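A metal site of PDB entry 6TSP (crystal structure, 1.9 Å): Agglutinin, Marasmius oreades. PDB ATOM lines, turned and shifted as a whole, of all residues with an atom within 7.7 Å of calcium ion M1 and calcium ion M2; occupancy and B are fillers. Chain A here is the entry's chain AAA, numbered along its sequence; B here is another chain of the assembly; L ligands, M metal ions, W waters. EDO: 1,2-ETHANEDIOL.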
ATOM      1  N   TRP A 208      -8.844   4.738  -8.657  1.00  0.00           N
ATOM      2  CA  TRP A 208     -10.067   5.494  -8.310  1.00  0.00           C
ATOM      3  C   TRP A 208      -9.752   6.470  -7.178  1.00  0.00           C
ATOM      4  O   TRP A 208      -9.232   6.033  -6.168  1.00  0.00           O
ATOM      5  CB  TRP A 208     -11.198   4.530  -7.923  1.00  0.00           C
ATOM      6  CG  TRP A 208     -12.507   5.208  -7.652  1.00  0.00           C
ATOM      7  CD1 TRP A 208     -13.551   5.370  -8.523  1.00  0.00           C
ATOM      8  CD2 TRP A 208     -12.910   5.857  -6.432  1.00  0.00           C
ATOM      9  NE1 TRP A 208     -14.572   6.056  -7.926  1.00  0.00           N
ATOM     10  CE2 TRP A 208     -14.217   6.355  -6.631  1.00  0.00           C
ATOM     11  CE3 TRP A 208     -12.313   6.030  -5.169  1.00  0.00           C
ATOM     12  CZ2 TRP A 208     -14.921   7.021  -5.638  1.00  0.00           C
ATOM     13  CZ3 TRP A 208     -13.015   6.709  -4.191  1.00  0.00           C
ATOM     14  CH2 TRP A 208     -14.295   7.193  -4.426  1.00  0.00           C
ATOM     15  N   ARG A 209     -10.043   7.748  -7.390  1.00  0.00           N
ATOM     16  CA  ARG A 209      -9.923   8.798  -6.345  1.00  0.00           C
ATOM     17  C   ARG A 209     -11.182   9.682  -6.366  1.00  0.00           C
ATOM     18  O   ARG A 209     -11.670  10.026  -7.492  1.00  0.00           O
ATOM     19  CB  ARG A 209      -8.647   9.615  -6.566  1.00  0.00           C
ATOM     20  CG  ARG A 209      -7.373   8.775  -6.598  1.00  0.00           C
ATOM     21  CD  ARG A 209      -6.129   9.584  -7.079  1.00  0.00           C
ATOM     22  NE  ARG A 209      -5.964  10.800  -6.310  1.00  0.00           N
ATOM     23  CZ  ARG A 209      -5.223  11.861  -6.703  1.00  0.00           C
ATOM     24  NH1 ARG A 209      -4.488  11.794  -7.788  1.00  0.00           N
ATOM     25  NH2 ARG A 209      -5.181  12.944  -5.955  1.00  0.00           N
ATOM     26  N   GLU A 210     -11.754   9.917  -5.202  1.00  0.00           N
ATOM     27  CA  GLU A 210     -13.044  10.624  -5.061  1.00  0.00           C
ATOM     28  C   GLU A 210     -13.007  11.952  -5.847  1.00  0.00           C
ATOM     29  O   GLU A 210     -12.135  12.822  -5.532  1.00  0.00           O
ATOM     30  CB  GLU A 210     -13.328  10.873  -3.580  1.00  0.00           C
ATOM     31  CG  GLU A 210     -14.749  11.231  -3.302  1.00  0.00           C
ATOM     32  CD  GLU A 210     -15.012  11.617  -1.859  1.00  0.00           C
ATOM     33  OE1 GLU A 210     -15.903  12.455  -1.634  1.00  0.00           O
ATOM     34  OE2 GLU A 210     -14.273  11.130  -0.978  1.00  0.00           O
ATOM     35  N   GLN A 211     -13.854  12.057  -6.881  1.00  0.00           N
ATOM     36  CA  GLN A 211     -14.074  13.255  -7.737  1.00  0.00           C
ATOM     37  C   GLN A 211     -12.830  13.479  -8.655  1.00  0.00           C
ATOM     38  O   GLN A 211     -13.029  13.804  -9.809  1.00  0.00           O
ATOM     39  CB  GLN A 211     -14.377  14.494  -6.874  1.00  0.00           C
ATOM     40  CG  GLN A 211     -15.749  14.416  -6.173  1.00  0.00           C
ATOM     41  CD  GLN A 211     -16.263  15.779  -5.726  1.00  0.00           C
ATOM     42  OE1 GLN A 211     -16.275  16.728  -6.498  1.00  0.00           O
ATOM     43  NE2 GLN A 211     -16.681  15.874  -4.468  1.00  0.00           N
ATOM     44  N   ILE A 212     -11.621  13.411  -8.096  1.00  0.00           N
ATOM     45  CA  ILE A 212     -10.400  13.889  -8.838  1.00  0.00           C
ATOM     46  C   ILE A 212     -10.053  12.868  -9.959  1.00  0.00           C
ATOM     47  O   ILE A 212      -9.491  13.297 -11.004  1.00  0.00           O
ATOM     48  CB  ILE A 212      -9.219  14.120  -7.879  1.00  0.00           C
ATOM     49  CG1 ILE A 212      -8.048  14.846  -8.585  1.00  0.00           C
ATOM     50  CG2 ILE A 212      -8.779  12.836  -7.249  1.00  0.00           C
ATOM     51  CD1 ILE A 212      -8.422  16.205  -9.146  1.00  0.00           C
ATOM     52  N   TYR A 213     -10.317  11.592  -9.718  1.00  0.00           N
ATOM     53  CA  TYR A 213     -10.244  10.559 -10.810  1.00  0.00           C
ATOM     54  C   TYR A 213     -11.184   9.404 -10.463  1.00  0.00           C
ATOM     55  O   TYR A 213     -10.720   8.324 -10.025  1.00  0.00           O
ATOM     56  CB  TYR A 213      -8.818  10.085 -11.002  1.00  0.00           C
ATOM     57  CG  TYR A 213      -8.456   9.870 -12.433  1.00  0.00           C
ATOM     58  CD1 TYR A 213      -8.311  10.938 -13.300  1.00  0.00           C
ATOM     59  CD2 TYR A 213      -8.378   8.591 -12.969  1.00  0.00           C
ATOM     60  CE1 TYR A 213      -8.031  10.758 -14.643  1.00  0.00           C
ATOM     61  CE2 TYR A 213      -8.093   8.381 -14.311  1.00  0.00           C
ATOM     62  CZ  TYR A 213      -7.934   9.470 -15.159  1.00  0.00           C
ATOM     63  OH  TYR A 213      -7.645   9.281 -16.495  1.00  0.00           O
ATOM     64  N   ASP A 214     -12.446   9.622 -10.674  1.00  0.00           N
ATOM     65  CA  ASP A 214     -13.501   8.641 -10.362  1.00  0.00           C
ATOM     66  C   ASP A 214     -14.164   8.265 -11.686  1.00  0.00           C
ATOM     67  O   ASP A 214     -13.475   8.345 -12.728  1.00  0.00           O
ATOM     68  CB  ASP A 214     -14.483   9.202  -9.326  1.00  0.00           C
ATOM     69  CG  ASP A 214     -15.271  10.424  -9.792  1.00  0.00           C
ATOM     70  OD1 ASP A 214     -14.716  11.195 -10.611  1.00  0.00           O
ATOM     71  OD2 ASP A 214     -16.397  10.608  -9.319  1.00  0.00           O
ATOM     72  N   CYS A 215     -15.333   7.655 -11.634  1.00  0.00           N
ATOM     73  CA  CYS A 215     -15.834   6.851 -12.781  1.00  0.00           C
ATOM     74  C   CYS A 215     -15.977   7.747 -14.047  1.00  0.00           C
ATOM     75  O   CYS A 215     -15.555   7.301 -15.104  1.00  0.00           O
ATOM     76  CB  CYS A 215     -17.180   6.146 -12.458  1.00  0.00           C
ATOM     77  SG  CYS A 215     -18.396   7.196 -11.620  1.00  0.00           S
ATOM     78  N   ASP A 216     -16.419   9.005 -13.895  1.00  0.00           N
ATOM     79  CA  ASP A 216     -16.574   9.931 -15.084  1.00  0.00           C
ATOM     80  C   ASP A 216     -15.184  10.120 -15.780  1.00  0.00           C
ATOM     81  O   ASP A 216     -15.147  10.113 -17.037  1.00  0.00           O
ATOM     82  CB  ASP A 216     -17.228  11.260 -14.706  1.00  0.00           C
ATOM     83  CG  ASP A 216     -16.581  11.951 -13.522  1.00  0.00           C
ATOM     84  OD1 ASP A 216     -16.976  11.659 -12.396  1.00  0.00           O
ATOM     85  OD2 ASP A 216     -15.679  12.776 -13.745  1.00  0.00           O
ATOM     86  N   ASP A 217     -14.087  10.122 -15.000  1.00  0.00           N
ATOM     87  CA  ASP A 217     -12.718  10.392 -15.523  1.00  0.00           C
ATOM     88  C   ASP A 217     -12.205   9.171 -16.284  1.00  0.00           C
ATOM     89  O   ASP A 217     -11.655   9.353 -17.397  1.00  0.00           O
ATOM     90  CB  ASP A 217     -11.777  10.782 -14.385  1.00  0.00           C
ATOM     91  CG  ASP A 217     -12.150  12.081 -13.728  1.00  0.00           C
ATOM     92  OD1 ASP A 217     -11.894  13.150 -14.345  1.00  0.00           O
ATOM     93  OD2 ASP A 217     -12.887  12.028 -12.721  1.00  0.00           O
ATOM     94  N   PHE A 218     -12.518   7.965 -15.790  1.00  0.00           N
ATOM     95  CA  PHE A 218     -12.152   6.694 -16.477  1.00  0.00           C
ATOM     96  C   PHE A 218     -12.901   6.610 -17.823  1.00  0.00           C
ATOM     97  O   PHE A 218     -12.270   6.314 -18.823  1.00  0.00           O
ATOM     98  CB  PHE A 218     -12.469   5.490 -15.585  1.00  0.00           C
ATOM     99  CG  PHE A 218     -11.421   5.181 -14.548  1.00  0.00           C
ATOM    100  CD1 PHE A 218     -11.405   5.852 -13.323  1.00  0.00           C
ATOM    101  CD2 PHE A 218     -10.498   4.161 -14.741  1.00  0.00           C
ATOM    102  CE1 PHE A 218     -10.451   5.545 -12.359  1.00  0.00           C
ATOM    103  CE2 PHE A 218      -9.540   3.875 -13.786  1.00  0.00           C
ATOM    104  CZ  PHE A 218      -9.547   4.533 -12.573  1.00  0.00           C
ATOM    105  N   ILE A 220     -14.428   8.903 -19.712  1.00  0.00           N
ATOM    106  CA  ILE A 220     -14.095   9.970 -20.681  1.00  0.00           C
ATOM    107  C   ILE A 220     -12.652   9.755 -21.204  1.00  0.00           C
ATOM    108  O   ILE A 220     -12.457   9.892 -22.415  1.00  0.00           O
ATOM    109  CB  ILE A 220     -14.273  11.359 -20.048  1.00  0.00           C
ATOM    110  CG1 ILE A 220     -15.746  11.772 -20.005  1.00  0.00           C
ATOM    111  CG2 ILE A 220     -13.399  12.388 -20.772  1.00  0.00           C
ATOM    112  CD1 ILE A 220     -16.066  12.797 -18.971  1.00  0.00           C
ATOM    113  N   ALA A 256     -25.152   7.102  -8.974  1.00  0.00           N
ATOM    114  CA  ALA A 256     -24.850   7.212 -10.424  1.00  0.00           C
ATOM    115  C   ALA A 256     -23.435   6.690 -10.697  1.00  0.00           C
ATOM    116  O   ALA A 256     -22.602   6.714  -9.777  1.00  0.00           O
ATOM    117  CB  ALA A 256     -25.017   8.639 -10.879  1.00  0.00           C
ATOM    118  N   ALA A 258     -20.485   6.269 -14.173  1.00  0.00           N
ATOM    119  CA  ALA A 258     -20.085   6.481 -15.592  1.00  0.00           C
ATOM    120  C   ALA A 258     -19.352   5.243 -16.109  1.00  0.00           C
ATOM    121  O   ALA A 258     -18.628   4.621 -15.332  1.00  0.00           O
ATOM    122  CB  ALA A 258     -19.236   7.703 -15.704  1.00  0.00           C
ATOM    123  N   ILE B 181     -24.040  16.739 -14.813  1.00  0.00           N
ATOM    124  CA  ILE B 181     -23.071  17.063 -13.729  1.00  0.00           C
ATOM    125  C   ILE B 181     -22.346  15.788 -13.327  1.00  0.00           C
ATOM    126  O   ILE B 181     -23.018  14.767 -13.131  1.00  0.00           O
ATOM    127  CB  ILE B 181     -23.802  17.697 -12.541  1.00  0.00           C
ATOM    128  CG1 ILE B 181     -24.300  19.107 -12.871  1.00  0.00           C
ATOM    129  CG2 ILE B 181     -22.932  17.677 -11.286  1.00  0.00           C
ATOM    130  CD1 ILE B 181     -25.738  19.385 -12.452  1.00  0.00           C
ATOM    131  N   LEU B 182     -21.029  15.831 -13.257  1.00  0.00           N
ATOM    132  CA  LEU B 182     -20.178  14.636 -13.066  1.00  0.00           C
ATOM    133  C   LEU B 182     -19.613  14.626 -11.633  1.00  0.00           C
ATOM    134  O   LEU B 182     -19.309  13.540 -11.136  1.00  0.00           O
ATOM    135  CB  LEU B 182     -19.062  14.663 -14.113  1.00  0.00           C
ATOM    136  CG  LEU B 182     -19.523  14.633 -15.570  1.00  0.00           C
ATOM    137  CD1 LEU B 182     -18.347  14.751 -16.519  1.00  0.00           C
ATOM    138  CD2 LEU B 182     -20.333  13.382 -15.862  1.00  0.00           C
ATOM    139  N   ASP B 183     -19.371  15.801 -11.064  1.00  0.00           N
ATOM    140  CA  ASP B 183     -18.656  15.938  -9.755  1.00  0.00           C
ATOM    141  C   ASP B 183     -19.373  16.997  -8.901  1.00  0.00           C
ATOM    142  O   ASP B 183     -20.437  17.496  -9.340  1.00  0.00           O
ATOM    143  CB  ASP B 183     -17.175  16.256  -9.975  1.00  0.00           C
ATOM    144  CG  ASP B 183     -16.392  15.125 -10.700  1.00  0.00           C
ATOM    145  OD1 ASP B 183     -16.327  13.994 -10.145  1.00  0.00           O
ATOM    146  OD2 ASP B 183     -15.781  15.424 -11.759  1.00  0.00           O
ATOM    147  N   GLY B 184     -18.830  17.295  -7.708  1.00  0.00           N
ATOM    148  CA  GLY B 184     -19.504  18.144  -6.700  1.00  0.00           C
ATOM    149  C   GLY B 184     -18.813  19.505  -6.536  1.00  0.00           C
ATOM    150  O   GLY B 184     -19.489  20.448  -6.187  1.00  0.00           O
ATOM    151  N   TYR B 186     -15.344  21.905  -7.872  1.00  0.00           N
ATOM    152  CA  TYR B 186     -14.349  22.076  -8.964  1.00  0.00           C
ATOM    153  C   TYR B 186     -13.408  23.252  -8.645  1.00  0.00           C
ATOM    154  O   TYR B 186     -13.909  24.412  -8.568  1.00  0.00           O
ATOM    155  CB  TYR B 186     -15.045  22.315 -10.292  1.00  0.00           C
ATOM    156  CG  TYR B 186     -16.085  21.295 -10.659  1.00  0.00           C
ATOM    157  CD1 TYR B 186     -17.414  21.433 -10.258  1.00  0.00           C
ATOM    158  CD2 TYR B 186     -15.772  20.241 -11.521  1.00  0.00           C
ATOM    159  CE1 TYR B 186     -18.394  20.549 -10.687  1.00  0.00           C
ATOM    160  CE2 TYR B 186     -16.741  19.363 -11.958  1.00  0.00           C
ATOM    161  CZ  TYR B 186     -18.058  19.514 -11.544  1.00  0.00           C
ATOM    162  OH  TYR B 186     -19.015  18.654 -11.990  1.00  0.00           O
ATOM    163  N   LYS B 223     -11.026  17.826 -22.352  1.00  0.00           N
ATOM    164  CA  LYS B 223     -11.596  17.462 -21.028  1.00  0.00           C
ATOM    165  C   LYS B 223     -10.755  16.338 -20.380  1.00  0.00           C
ATOM    166  O   LYS B 223     -10.523  16.399 -19.182  1.00  0.00           O
ATOM    167  CB  LYS B 223     -13.059  17.029 -21.142  1.00  0.00           C
ATOM    168  CG  LYS B 223     -13.697  16.619 -19.811  1.00  0.00           C
ATOM    169  CD  LYS B 223     -15.124  17.033 -19.658  1.00  0.00           C
ATOM    170  CE  LYS B 223     -15.697  16.709 -18.286  1.00  0.00           C
ATOM    171  NZ  LYS B 223     -14.969  17.429 -17.201  1.00  0.00           N
ATOM    172  N   GLY B 227      -8.709  16.425 -16.859  1.00  0.00           N
ATOM    173  CA  GLY B 227      -8.881  15.295 -15.916  1.00  0.00           C
ATOM    174  C   GLY B 227      -7.531  14.691 -15.514  1.00  0.00           C
ATOM    175  O   GLY B 227      -7.285  14.509 -14.273  1.00  0.00           O
ATOM    176  N   PHE B 239     -12.363  16.601  -4.807  1.00  0.00           N
ATOM    177  CA  PHE B 239     -12.715  17.685  -5.734  1.00  0.00           C
ATOM    178  C   PHE B 239     -12.356  17.263  -7.158  1.00  0.00           C
ATOM    179  O   PHE B 239     -11.517  16.332  -7.296  1.00  0.00           O
ATOM    180  CB  PHE B 239     -11.978  18.968  -5.354  1.00  0.00           C
ATOM    181  CG  PHE B 239     -10.499  18.876  -5.518  1.00  0.00           C
ATOM    182  CD1 PHE B 239      -9.753  18.061  -4.679  1.00  0.00           C
ATOM    183  CD2 PHE B 239      -9.865  19.455  -6.612  1.00  0.00           C
ATOM    184  CE1 PHE B 239      -8.410  17.846  -4.934  1.00  0.00           C
ATOM    185  CE2 PHE B 239      -8.516  19.263  -6.833  1.00  0.00           C
ATOM    186  CZ  PHE B 239      -7.787  18.466  -5.995  1.00  0.00           C
ATOM    187  N   ALA B 240     -12.742  18.077  -8.122  1.00  0.00           N
ATOM    188  CA  ALA B 240     -12.372  17.912  -9.549  1.00  0.00           C
ATOM    189  C   ALA B 240     -11.800  19.225 -10.086  1.00  0.00           C
ATOM    190  O   ALA B 240     -11.850  20.242  -9.349  1.00  0.00           O
ATOM    191  CB  ALA B 240     -13.577  17.490 -10.331  1.00  0.00           C
ATOM    192  N   ILE B 241     -11.365  19.228 -11.336  1.00  0.00           N
ATOM    193  CA  ILE B 241     -10.956  20.464 -12.086  1.00  0.00           C
ATOM    194  C   ILE B 241     -12.080  20.843 -13.018  1.00  0.00           C
ATOM    195  O   ILE B 241     -12.585  19.958 -13.720  1.00  0.00           O
ATOM    196  CB  ILE B 241      -9.656  20.239 -12.856  1.00  0.00           C
ATOM    197  CG1 ILE B 241      -8.617  19.479 -12.022  1.00  0.00           C
ATOM    198  CG2 ILE B 241      -9.111  21.565 -13.370  1.00  0.00           C
ATOM    199  CD1 ILE B 241      -8.241  20.157 -10.704  1.00  0.00           C
ATOM    200  N   TYR B 293     -19.833  18.382 -17.428  1.00  0.00           N
ATOM    201  CA  TYR B 293     -18.754  19.038 -16.670  1.00  0.00           C
ATOM    202  C   TYR B 293     -18.684  18.413 -15.284  1.00  0.00           C
ATOM    203  O   TYR B 293     -17.616  18.342 -14.675  1.00  0.00           O
ATOM    204  CB  TYR B 293     -19.016  20.544 -16.565  1.00  0.00           C
ATOM    205  CG  TYR B 293     -20.405  20.920 -16.070  1.00  0.00           C
ATOM    206  CD1 TYR B 293     -21.476  21.043 -16.952  1.00  0.00           C
ATOM    207  CD2 TYR B 293     -20.626  21.219 -14.738  1.00  0.00           C
ATOM    208  CE1 TYR B 293     -22.727  21.472 -16.518  1.00  0.00           C
ATOM    209  CE2 TYR B 293     -21.883  21.601 -14.278  1.00  0.00           C
ATOM    210  CZ  TYR B 293     -22.931  21.748 -15.177  1.00  0.00           C
ATOM    211  OH  TYR B 293     -24.163  22.168 -14.736  1.00  0.00           O
ATOM    212  OXT TYR B 293     -19.688  17.956 -14.768  1.00  0.00           O
HETATM  213  C1  EDO L   1     -20.519  10.327 -12.768  1.00  0.00           C
HETATM  214  O1  EDO L   1     -21.709  10.729 -13.434  1.00  0.00           O
HETATM  215  C2  EDO L   1     -20.705  10.172 -11.293  1.00  0.00           C
HETATM  216  O2  EDO L   1     -19.501  10.289 -10.576  1.00  0.00           O
HETATM  217 CA    CA M   1     -17.876  12.079 -10.298  1.00  0.00          CA
HETATM  218 CA    CA M   2     -14.427  13.286 -11.695  1.00  0.00          CA
HETATM  219 ZN    ZN M   3     -18.809   5.231 -10.346  1.00  0.00          ZN
HETATM  220  O   HOH W   1     -13.296  14.870 -13.002  1.00  0.00           O
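Calcium ion M1 is bound by O of Leu 182 of chain B (2.2 Å), OD2 of Asp 214 (2.3 Å), OD1 of Asp 216 (2.3 Å), O2 of the ligand (2.4 Å) and OD1 of Asp 183 of chain B (2.5 Å). Calcium ion M1 has five donor atoms within binding distance.
OD2 of Asp 217 binds calcium ion M2, at 2.2 Å. Calcium ion M2 is bound by water W1. OD1 of Asp 214 is bound to calcium ion M2 (2.4 Å). Calcium ion M2 is bound by O of Gln 211 (2.4 Å). The side-chain carboxylate (OD2) of Asp 216 is bound to calcium ion M2 (2.5 Å). The side-chain carboxylate (OD2) of Asp 183 of chain B is bound to calcium ion M2 (2.5 Å). OD1 of Asp 183 of chain B binds calcium ion M2, at 2.6 Å. Calcium ion M2 has seven donor atoms within binding distance. Slightly farther from calcium ion M2 lies the side-chain carboxylate (OD1) of Asp 216 (3.1 Å).
The backbone NH (N) of Gly 184 of chain B sits at hydrogen-bond distance from the side-chain amide oxygen (OE1) of Gln 211 (2.9 Å). The backbone carbonyl oxygen (O) of Arg 209 sits at hydrogen-bond distance from the backbone NH (N) of Asp 214 (3.3 Å). OH of Tyr 186 of chain B is in hydrogen-bond range of N of Asp 183 of chain B, at 3.0 Å. The backbone NH of Leu 182 of chain B is in hydrogen-bond range of the chain-end carboxylate of Tyr 293 of chain B.
Of the 25 residues printed, 5 come within 4 Å of calcium ion M2. The nearest printed residue that does not touch calcium ion M2 is Ala 240 of chain B (4.5 Å).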
